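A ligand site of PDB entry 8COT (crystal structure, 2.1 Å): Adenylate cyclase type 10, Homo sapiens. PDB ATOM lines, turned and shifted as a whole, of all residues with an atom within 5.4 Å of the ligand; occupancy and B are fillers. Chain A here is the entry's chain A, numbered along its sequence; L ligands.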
ATOM      1  N   PHE A  45     -18.635  19.769  -6.509  1.00  0.00           N
ATOM      2  CA  PHE A  45     -19.579  18.972  -7.274  1.00  0.00           C
ATOM      3  C   PHE A  45     -20.242  18.008  -6.312  1.00  0.00           C
ATOM      4  O   PHE A  45     -19.563  17.177  -5.700  1.00  0.00           O
ATOM      5  CB  PHE A  45     -18.876  18.218  -8.397  1.00  0.00           C
ATOM      6  CG  PHE A  45     -19.823  17.619  -9.400  1.00  0.00           C
ATOM      7  CD1 PHE A  45     -20.674  18.424 -10.142  1.00  0.00           C
ATOM      8  CD2 PHE A  45     -19.851  16.260  -9.606  1.00  0.00           C
ATOM      9  CE1 PHE A  45     -21.537  17.873 -11.064  1.00  0.00           C
ATOM     10  CE2 PHE A  45     -20.708  15.700 -10.528  1.00  0.00           C
ATOM     11  CZ  PHE A  45     -21.556  16.509 -11.261  1.00  0.00           C
ATOM     12  N   LEU A  94     -23.602  27.109  -9.743  1.00  0.00           N
ATOM     13  CA  LEU A  94     -23.510  27.432 -11.159  1.00  0.00           C
ATOM     14  C   LEU A  94     -24.628  26.782 -11.966  1.00  0.00           C
ATOM     15  O   LEU A  94     -25.305  27.460 -12.743  1.00  0.00           O
ATOM     16  CB  LEU A  94     -22.144  27.005 -11.694  1.00  0.00           C
ATOM     17  CG  LEU A  94     -20.930  27.771 -11.154  1.00  0.00           C
ATOM     18  CD1 LEU A  94     -19.691  27.262 -11.878  1.00  0.00           C
ATOM     19  CD2 LEU A  94     -21.076  29.265 -11.326  1.00  0.00           C
ATOM     20  N   LYS A  95     -24.849  25.479 -11.782  1.00  0.00           N
ATOM     21  CA  LYS A  95     -25.843  24.780 -12.572  1.00  0.00           C
ATOM     22  C   LYS A  95     -26.387  23.596 -11.783  1.00  0.00           C
ATOM     23  O   LYS A  95     -25.700  23.049 -10.920  1.00  0.00           O
ATOM     24  CB  LYS A  95     -25.268  24.252 -13.895  1.00  0.00           C
ATOM     25  CG  LYS A  95     -25.632  25.068 -15.113  1.00  0.00           C
ATOM     26  CD  LYS A  95     -24.975  24.538 -16.381  1.00  0.00           C
ATOM     27  CE  LYS A  95     -24.490  25.690 -17.259  1.00  0.00           C
ATOM     28  NZ  LYS A  95     -24.427  25.335 -18.694  1.00  0.00           N
ATOM     29  N   PHE A  96     -27.616  23.205 -12.107  1.00  0.00           N
ATOM     30  CA  PHE A  96     -28.234  22.001 -11.592  1.00  0.00           C
ATOM     31  C   PHE A  96     -28.344  20.970 -12.707  1.00  0.00           C
ATOM     32  O   PHE A  96     -28.570  21.307 -13.868  1.00  0.00           O
ATOM     33  CB  PHE A  96     -29.652  22.274 -11.067  1.00  0.00           C
ATOM     34  CG  PHE A  96     -29.700  23.092  -9.816  1.00  0.00           C
ATOM     35  CD1 PHE A  96     -29.773  24.473  -9.887  1.00  0.00           C
ATOM     36  CD2 PHE A  96     -29.708  22.478  -8.566  1.00  0.00           C
ATOM     37  CE1 PHE A  96     -29.831  25.230  -8.738  1.00  0.00           C
ATOM     38  CE2 PHE A  96     -29.770  23.231  -7.426  1.00  0.00           C
ATOM     39  CZ  PHE A  96     -29.836  24.617  -7.501  1.00  0.00           C
ATOM     40  N   ALA A  97     -28.204  19.701 -12.336  1.00  0.00           N
ATOM     41  CA  ALA A  97     -28.599  18.597 -13.203  1.00  0.00           C
ATOM     42  C   ALA A  97     -29.343  17.586 -12.337  1.00  0.00           C
ATOM     43  O   ALA A  97     -29.247  17.612 -11.111  1.00  0.00           O
ATOM     44  CB  ALA A  97     -27.400  17.933 -13.884  1.00  0.00           C
ATOM     45  N   ASP A  99     -28.557  14.616 -11.709  1.00  0.00           N
ATOM     46  CA  ASP A  99     -27.644  13.843 -10.892  1.00  0.00           C
ATOM     47  C   ASP A  99     -26.748  14.690  -9.982  1.00  0.00           C
ATOM     48  O   ASP A  99     -26.089  14.114  -9.106  1.00  0.00           O
ATOM     49  CB  ASP A  99     -26.768  12.942 -11.784  1.00  0.00           C
ATOM     50  CG  ASP A  99     -26.130  13.697 -12.936  1.00  0.00           C
ATOM     51  OD1 ASP A  99     -26.666  14.756 -13.329  1.00  0.00           O
ATOM     52  OD2 ASP A  99     -25.103  13.219 -13.451  1.00  0.00           O
ATOM     53  N   ALA A 100     -26.702  16.011 -10.146  1.00  0.00           N
ATOM     54  CA  ALA A 100     -25.774  16.778  -9.315  1.00  0.00           C
ATOM     55  C   ALA A 100     -26.044  18.282  -9.384  1.00  0.00           C
ATOM     56  O   ALA A 100     -26.966  18.760 -10.060  1.00  0.00           O
ATOM     57  CB  ALA A 100     -24.332  16.491  -9.741  1.00  0.00           C
ATOM     58  N   LEU A 101     -25.219  19.035  -8.651  1.00  0.00           N
ATOM     59  CA  LEU A 101     -25.087  20.472  -8.807  1.00  0.00           C
ATOM     60  C   LEU A 101     -23.611  20.832  -8.662  1.00  0.00           C
ATOM     61  O   LEU A 101     -22.867  20.196  -7.910  1.00  0.00           O
ATOM     62  CB  LEU A 101     -25.926  21.260  -7.808  1.00  0.00           C
ATOM     63  CG  LEU A 101     -25.565  21.273  -6.318  1.00  0.00           C
ATOM     64  CD1 LEU A 101     -24.490  22.302  -6.036  1.00  0.00           C
ATOM     65  CD2 LEU A 101     -26.818  21.553  -5.499  1.00  0.00           C
ATOM     66  N   LEU A 102     -23.207  21.871  -9.386  1.00  0.00           N
ATOM     67  CA  LEU A 102     -21.830  22.374  -9.354  1.00  0.00           C
ATOM     68  C   LEU A 102     -21.842  23.768  -8.754  1.00  0.00           C
ATOM     69  O   LEU A 102     -22.643  24.619  -9.138  1.00  0.00           O
ATOM     70  CB  LEU A 102     -21.230  22.418 -10.756  1.00  0.00           C
ATOM     71  CG  LEU A 102     -19.834  23.016 -10.922  1.00  0.00           C
ATOM     72  CD1 LEU A 102     -18.774  22.120 -10.329  1.00  0.00           C
ATOM     73  CD2 LEU A 102     -19.567  23.280 -12.412  1.00  0.00           C
ATOM     74  N   PHE A 165     -23.641  29.325 -20.781  1.00  0.00           N
ATOM     75  CA  PHE A 165     -22.303  29.468 -20.228  1.00  0.00           C
ATOM     76  C   PHE A 165     -21.772  28.126 -19.736  1.00  0.00           C
ATOM     77  O   PHE A 165     -22.519  27.180 -19.469  1.00  0.00           O
ATOM     78  CB  PHE A 165     -22.262  30.503 -19.092  1.00  0.00           C
ATOM     79  CG  PHE A 165     -22.893  30.024 -17.813  1.00  0.00           C
ATOM     80  CD1 PHE A 165     -24.263  30.089 -17.644  1.00  0.00           C
ATOM     81  CD2 PHE A 165     -22.110  29.502 -16.795  1.00  0.00           C
ATOM     82  CE1 PHE A 165     -24.845  29.634 -16.469  1.00  0.00           C
ATOM     83  CE2 PHE A 165     -22.687  29.063 -15.617  1.00  0.00           C
ATOM     84  CZ  PHE A 165     -24.057  29.126 -15.470  1.00  0.00           C
ATOM     85  N   LEU A 166     -20.451  28.073 -19.617  1.00  0.00           N
ATOM     86  CA  LEU A 166     -19.733  26.926 -19.102  1.00  0.00           C
ATOM     87  C   LEU A 166     -18.532  27.425 -18.324  1.00  0.00           C
ATOM     88  O   LEU A 166     -18.041  28.541 -18.556  1.00  0.00           O
ATOM     89  CB  LEU A 166     -19.266  25.984 -20.215  1.00  0.00           C
ATOM     90  CG  LEU A 166     -20.301  25.288 -21.079  1.00  0.00           C
ATOM     91  CD1 LEU A 166     -19.643  24.770 -22.353  1.00  0.00           C
ATOM     92  CD2 LEU A 166     -20.953  24.152 -20.304  1.00  0.00           C
ATOM     93  N   VAL A 167     -18.044  26.596 -17.421  1.00  0.00           N
ATOM     94  CA  VAL A 167     -16.699  26.743 -16.872  1.00  0.00           C
ATOM     95  C   VAL A 167     -15.840  25.637 -17.465  1.00  0.00           C
ATOM     96  O   VAL A 167     -16.318  24.521 -17.711  1.00  0.00           O
ATOM     97  CB  VAL A 167     -16.665  26.726 -15.330  1.00  0.00           C
ATOM     98  CG1 VAL A 167     -17.044  28.093 -14.788  1.00  0.00           C
ATOM     99  CG2 VAL A 167     -17.585  25.638 -14.795  1.00  0.00           C
ATOM    100  N   ILE A 168     -14.573  25.966 -17.713  1.00  0.00           N
ATOM    101  CA  ILE A 168     -13.659  25.113 -18.453  1.00  0.00           C
ATOM    102  C   ILE A 168     -12.302  25.157 -17.765  1.00  0.00           C
ATOM    103  O   ILE A 168     -11.939  26.142 -17.119  1.00  0.00           O
ATOM    104  CB  ILE A 168     -13.525  25.579 -19.920  1.00  0.00           C
ATOM    105  CG1 ILE A 168     -14.863  25.484 -20.644  1.00  0.00           C
ATOM    106  CG2 ILE A 168     -12.468  24.771 -20.653  1.00  0.00           C
ATOM    107  CD1 ILE A 168     -14.916  26.295 -21.929  1.00  0.00           C
ATOM    108  N   VAL A 172     -11.867  22.265 -13.469  1.00  0.00           N
ATOM    109  CA  VAL A 172     -13.158  21.669 -13.766  1.00  0.00           C
ATOM    110  C   VAL A 172     -13.014  20.169 -14.002  1.00  0.00           C
ATOM    111  O   VAL A 172     -13.761  19.363 -13.448  1.00  0.00           O
ATOM    112  CB  VAL A 172     -13.799  22.376 -14.984  1.00  0.00           C
ATOM    113  CG1 VAL A 172     -15.129  21.740 -15.329  1.00  0.00           C
ATOM    114  CG2 VAL A 172     -13.960  23.868 -14.701  1.00  0.00           C
ATOM    115  N   ASP A 173     -12.047  19.774 -14.838  1.00  0.00           N
ATOM    116  CA  ASP A 173     -11.799  18.346 -15.023  1.00  0.00           C
ATOM    117  C   ASP A 173     -11.389  17.697 -13.715  1.00  0.00           C
ATOM    118  O   ASP A 173     -11.713  16.523 -13.472  1.00  0.00           O
ATOM    119  CB  ASP A 173     -10.714  18.132 -16.079  1.00  0.00           C
ATOM    120  CG  ASP A 173     -11.081  18.722 -17.432  1.00  0.00           C
ATOM    121  OD1 ASP A 173     -12.279  18.658 -17.802  1.00  0.00           O
ATOM    122  OD2 ASP A 173     -10.186  19.246 -18.114  1.00  0.00           O
ATOM    123  N   VAL A 175     -12.486  18.410 -10.633  1.00  0.00           N
ATOM    124  CA  VAL A 175     -13.651  18.114  -9.813  1.00  0.00           C
ATOM    125  C   VAL A 175     -14.435  16.965 -10.438  1.00  0.00           C
ATOM    126  O   VAL A 175     -15.097  16.201  -9.729  1.00  0.00           O
ATOM    127  CB  VAL A 175     -14.504  19.388  -9.628  1.00  0.00           C
ATOM    128  CG1 VAL A 175     -15.383  19.642 -10.851  1.00  0.00           C
ATOM    129  CG2 VAL A 175     -15.326  19.287  -8.355  1.00  0.00           C
ATOM    130  N   ARG A 176     -14.353  16.822 -11.763  1.00  0.00           N
ATOM    131  CA  ARG A 176     -14.900  15.644 -12.446  1.00  0.00           C
ATOM    132  C   ARG A 176     -14.391  14.370 -11.793  1.00  0.00           C
ATOM    133  O   ARG A 176     -15.156  13.575 -11.234  1.00  0.00           O
ATOM    134  CB  ARG A 176     -14.491  15.690 -13.920  1.00  0.00           C
ATOM    135  CG  ARG A 176     -15.355  14.907 -14.905  1.00  0.00           C
ATOM    136  CD  ARG A 176     -15.617  13.462 -14.495  1.00  0.00           C
ATOM    137  NE  ARG A 176     -15.944  12.645 -15.658  1.00  0.00           N
ATOM    138  CZ  ARG A 176     -16.474  11.422 -15.590  1.00  0.00           C
ATOM    139  NH1 ARG A 176     -16.742  10.754 -16.697  1.00  0.00           N
ATOM    140  NH2 ARG A 176     -16.764  10.894 -14.412  1.00  0.00           N
ATOM    141  N   GLN A 179     -15.010  13.653  -8.136  1.00  0.00           N
ATOM    142  CA  GLN A 179     -16.369  13.155  -7.909  1.00  0.00           C
ATOM    143  C   GLN A 179     -16.484  11.681  -8.276  1.00  0.00           C
ATOM    144  O   GLN A 179     -17.146  10.916  -7.567  1.00  0.00           O
ATOM    145  CB  GLN A 179     -17.369  13.979  -8.727  1.00  0.00           C
ATOM    146  CG  GLN A 179     -18.658  13.236  -9.086  1.00  0.00           C
ATOM    147  CD  GLN A 179     -18.669  12.714 -10.515  1.00  0.00           C
ATOM    148  OE1 GLN A 179     -18.105  13.342 -11.418  1.00  0.00           O
ATOM    149  NE2 GLN A 179     -19.315  11.575 -10.729  1.00  0.00           N
ATOM    150  N   PHE A 296     -28.953  13.808 -26.953  1.00  0.00           N
ATOM    151  CA  PHE A 296     -27.788  14.200 -26.164  1.00  0.00           C
ATOM    152  C   PHE A 296     -26.582  14.263 -27.103  1.00  0.00           C
ATOM    153  O   PHE A 296     -26.102  13.241 -27.579  1.00  0.00           O
ATOM    154  CB  PHE A 296     -27.561  13.218 -25.028  1.00  0.00           C
ATOM    155  CG  PHE A 296     -27.221  13.874 -23.715  1.00  0.00           C
ATOM    156  CD1 PHE A 296     -26.303  14.905 -23.651  1.00  0.00           C
ATOM    157  CD2 PHE A 296     -27.844  13.464 -22.539  1.00  0.00           C
ATOM    158  CE1 PHE A 296     -26.000  15.518 -22.446  1.00  0.00           C
ATOM    159  CE2 PHE A 296     -27.534  14.057 -21.341  1.00  0.00           C
ATOM    160  CZ  PHE A 296     -26.613  15.090 -21.290  1.00  0.00           C
ATOM    161  N   VAL A 335     -26.298  22.464 -20.906  1.00  0.00           N
ATOM    162  CA  VAL A 335     -24.999  22.321 -21.565  1.00  0.00           C
ATOM    163  C   VAL A 335     -23.961  22.016 -20.506  1.00  0.00           C
ATOM    164  O   VAL A 335     -23.920  22.686 -19.465  1.00  0.00           O
ATOM    165  CB  VAL A 335     -24.616  23.579 -22.362  1.00  0.00           C
ATOM    166  CG1 VAL A 335     -23.425  23.278 -23.248  1.00  0.00           C
ATOM    167  CG2 VAL A 335     -25.792  24.060 -23.198  1.00  0.00           C
ATOM    168  N   PHE A 336     -23.120  21.016 -20.766  1.00  0.00           N
ATOM    169  CA  PHE A 336     -22.077  20.596 -19.853  1.00  0.00           C
ATOM    170  C   PHE A 336     -20.755  20.509 -20.603  1.00  0.00           C
ATOM    171  O   PHE A 336     -20.727  20.432 -21.834  1.00  0.00           O
ATOM    172  CB  PHE A 336     -22.336  19.215 -19.234  1.00  0.00           C
ATOM    173  CG  PHE A 336     -23.659  19.081 -18.575  1.00  0.00           C
ATOM    174  CD1 PHE A 336     -24.067  19.980 -17.604  1.00  0.00           C
ATOM    175  CD2 PHE A 336     -24.504  18.031 -18.915  1.00  0.00           C
ATOM    176  CE1 PHE A 336     -25.301  19.840 -16.998  1.00  0.00           C
ATOM    177  CE2 PHE A 336     -25.732  17.882 -18.308  1.00  0.00           C
ATOM    178  CZ  PHE A 336     -26.133  18.786 -17.343  1.00  0.00           C
ATOM    179  N   MET A 337     -19.665  20.480 -19.852  1.00  0.00           N
ATOM    180  CA  MET A 337     -18.349  20.257 -20.440  1.00  0.00           C
ATOM    181  C   MET A 337     -17.431  19.609 -19.415  1.00  0.00           C
ATOM    182  O   MET A 337     -17.131  20.208 -18.379  1.00  0.00           O
ATOM    183  CB  MET A 337     -17.734  21.566 -20.947  1.00  0.00           C
ATOM    184  CG  MET A 337     -16.283  21.429 -21.388  1.00  0.00           C
ATOM    185  SD  MET A 337     -15.965  22.122 -23.019  1.00  0.00           S
ATOM    186  CE  MET A 337     -14.649  21.028 -23.592  1.00  0.00           C
ATOM    187  N   PHE A 338     -16.996  18.379 -19.708  1.00  0.00           N
ATOM    188  CA  PHE A 338     -15.943  17.730 -18.936  1.00  0.00           C
ATOM    189  C   PHE A 338     -15.308  16.671 -19.838  1.00  0.00           C
ATOM    190  O   PHE A 338     -15.867  16.286 -20.865  1.00  0.00           O
ATOM    191  CB  PHE A 338     -16.466  17.094 -17.638  1.00  0.00           C
ATOM    192  CG  PHE A 338     -17.609  16.136 -17.821  1.00  0.00           C
ATOM    193  CD1 PHE A 338     -18.906  16.609 -17.972  1.00  0.00           C
ATOM    194  CD2 PHE A 338     -17.396  14.770 -17.812  1.00  0.00           C
ATOM    195  CE1 PHE A 338     -19.960  15.735 -18.113  1.00  0.00           C
ATOM    196  CE2 PHE A 338     -18.438  13.892 -17.958  1.00  0.00           C
ATOM    197  CZ  PHE A 338     -19.730  14.368 -18.100  1.00  0.00           C
ATOM    198  N   ASN A 412     -30.329   9.456 -18.690  1.00  0.00           N
ATOM    199  CA  ASN A 412     -29.048   8.801 -18.426  1.00  0.00           C
ATOM    200  C   ASN A 412     -28.665   7.886 -19.578  1.00  0.00           C
ATOM    201  O   ASN A 412     -27.485   7.815 -19.960  1.00  0.00           O
ATOM    202  CB  ASN A 412     -29.111   8.024 -17.122  1.00  0.00           C
ATOM    203  CG  ASN A 412     -29.529   8.906 -15.951  1.00  0.00           C
ATOM    204  OD1 ASN A 412     -29.331  10.121 -15.973  1.00  0.00           O
ATOM    205  ND2 ASN A 412     -30.125   8.289 -14.931  1.00  0.00           N
ATOM    206  N   ALA A 415     -27.231   9.871 -22.388  1.00  0.00           N
ATOM    207  CA  ALA A 415     -25.894  10.289 -21.987  1.00  0.00           C
ATOM    208  C   ALA A 415     -24.894   9.141 -22.091  1.00  0.00           C
ATOM    209  O   ALA A 415     -23.758   9.335 -22.541  1.00  0.00           O
ATOM    210  CB  ALA A 415     -25.934  10.850 -20.559  1.00  0.00           C
HETATM  211  C1  LIG L   1     -19.386  22.785 -16.896  1.00  0.00           C
HETATM  212  C2  LIG L   1     -21.315  21.987 -15.441  1.00  0.00           C
HETATM  213  C3  LIG L   1     -21.698  23.404 -15.187  1.00  0.00           C
HETATM  214  C4  LIG L   1     -20.889  24.485 -15.806  1.00  0.00           C
HETATM  215  C5  LIG L   1     -22.154  20.886 -14.823  1.00  0.00           C
HETATM  216  C6  LIG L   1     -22.060  19.525 -14.994  1.00  0.00           C
HETATM  217  C7  LIG L   1     -23.040  18.940 -14.235  1.00  0.00           C
HETATM  218  C8  LIG L   1     -17.322  19.139 -14.325  1.00  0.00           C
HETATM  219  C9  LIG L   1     -18.576  19.427 -15.144  1.00  0.00           C
HETATM  220  C10 LIG L   1     -19.783  18.505 -15.062  1.00  0.00           C
HETATM  221  C11 LIG L   1     -19.726  17.276 -14.161  1.00  0.00           C
HETATM  222  C12 LIG L   1     -18.472  16.976 -13.350  1.00  0.00           C
HETATM  223  C13 LIG L   1     -17.266  17.910 -13.423  1.00  0.00           C
HETATM  224  C14 LIG L   1     -23.347  17.447 -14.102  1.00  0.00           C
HETATM  225  C15 LIG L   1     -22.907  15.815 -15.795  1.00  0.00           C
HETATM  226  C16 LIG L   1     -24.034  14.813 -15.534  1.00  0.00           C
HETATM  227  C17 LIG L   1     -24.261  13.943 -17.748  1.00  0.00           C
HETATM  228  C18 LIG L   1     -26.168  14.146 -16.358  1.00  0.00           C
HETATM  229  C19 LIG L   1     -21.042  18.802 -15.882  1.00  0.00           C
HETATM  230  C20 LIG L   1     -24.835  19.788 -12.701  1.00  0.00           C
HETATM  231  N1  LIG L   1     -19.765  24.180 -16.635  1.00  0.00           N
HETATM  232  N2  LIG L   1     -20.174  21.692 -16.294  1.00  0.00           N
HETATM  233  N3  LIG L   1     -23.708  19.921 -13.616  1.00  0.00           N
HETATM  234  N4  LIG L   1     -23.152  21.130 -13.985  1.00  0.00           N
HETATM  235  N5  LIG L   1     -24.897  14.735 -16.708  1.00  0.00           N
HETATM  236  N6  LIG L   1     -18.235  22.545 -17.727  1.00  0.00           N
HETATM  237  O1  LIG L   1     -22.493  16.451 -14.606  1.00  0.00           O
HETATM  238  O2  LIG L   1     -24.338  17.104 -13.536  1.00  0.00           O
HETATM  239 CL1  LIG L   1     -21.263  26.194 -15.562  1.00  0.00          CL
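O of Val 167 lies within hydrogen-bond range of N6 of the ligand.
A nitrogen (N1) of the ligand is in hydrogen-bond range of the backbone NH of Val 167 (3.1 Å).
O of Met 337 lies within hydrogen-bond range of N6 of the ligand, 2.7 Å away.
The side-chain carboxylate (OD2) of Asp 99 is in salt-bridge range of a nitrogen (N5) of the ligand (3.6 Å).
The backbone carbonyl oxygen (O) of Leu 102 lies within hydrogen-bond range of the backbone NH (N) of Leu 94.
N of Leu 102 sits at hydrogen-bond distance from O of Lys 95, 3.2 Å away.
The backbone carbonyl oxygen of Val 335 lies within hydrogen-bond range of the side-chain amino group of Lys 95 (2.8 Å).
The side-chain amino group (NZ) of Lys 95 lies within hydrogen-bond range of the backbone carbonyl oxygen (O) of Phe 165.
O of Arg 176 sits close to OE1 of Gln 179 (3.0 Å).
Residues that only touch the ligand: Ala 97, Phe 165, Phe 336, Arg 176, Phe 45, Leu 102, Ala 100, Val 172, Phe 338, Val 175, Lys 95, Leu 166, Phe 96 and Leu 101.
The nearest printed residue that does not touch the ligand is Leu 94 (4.05 Å).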
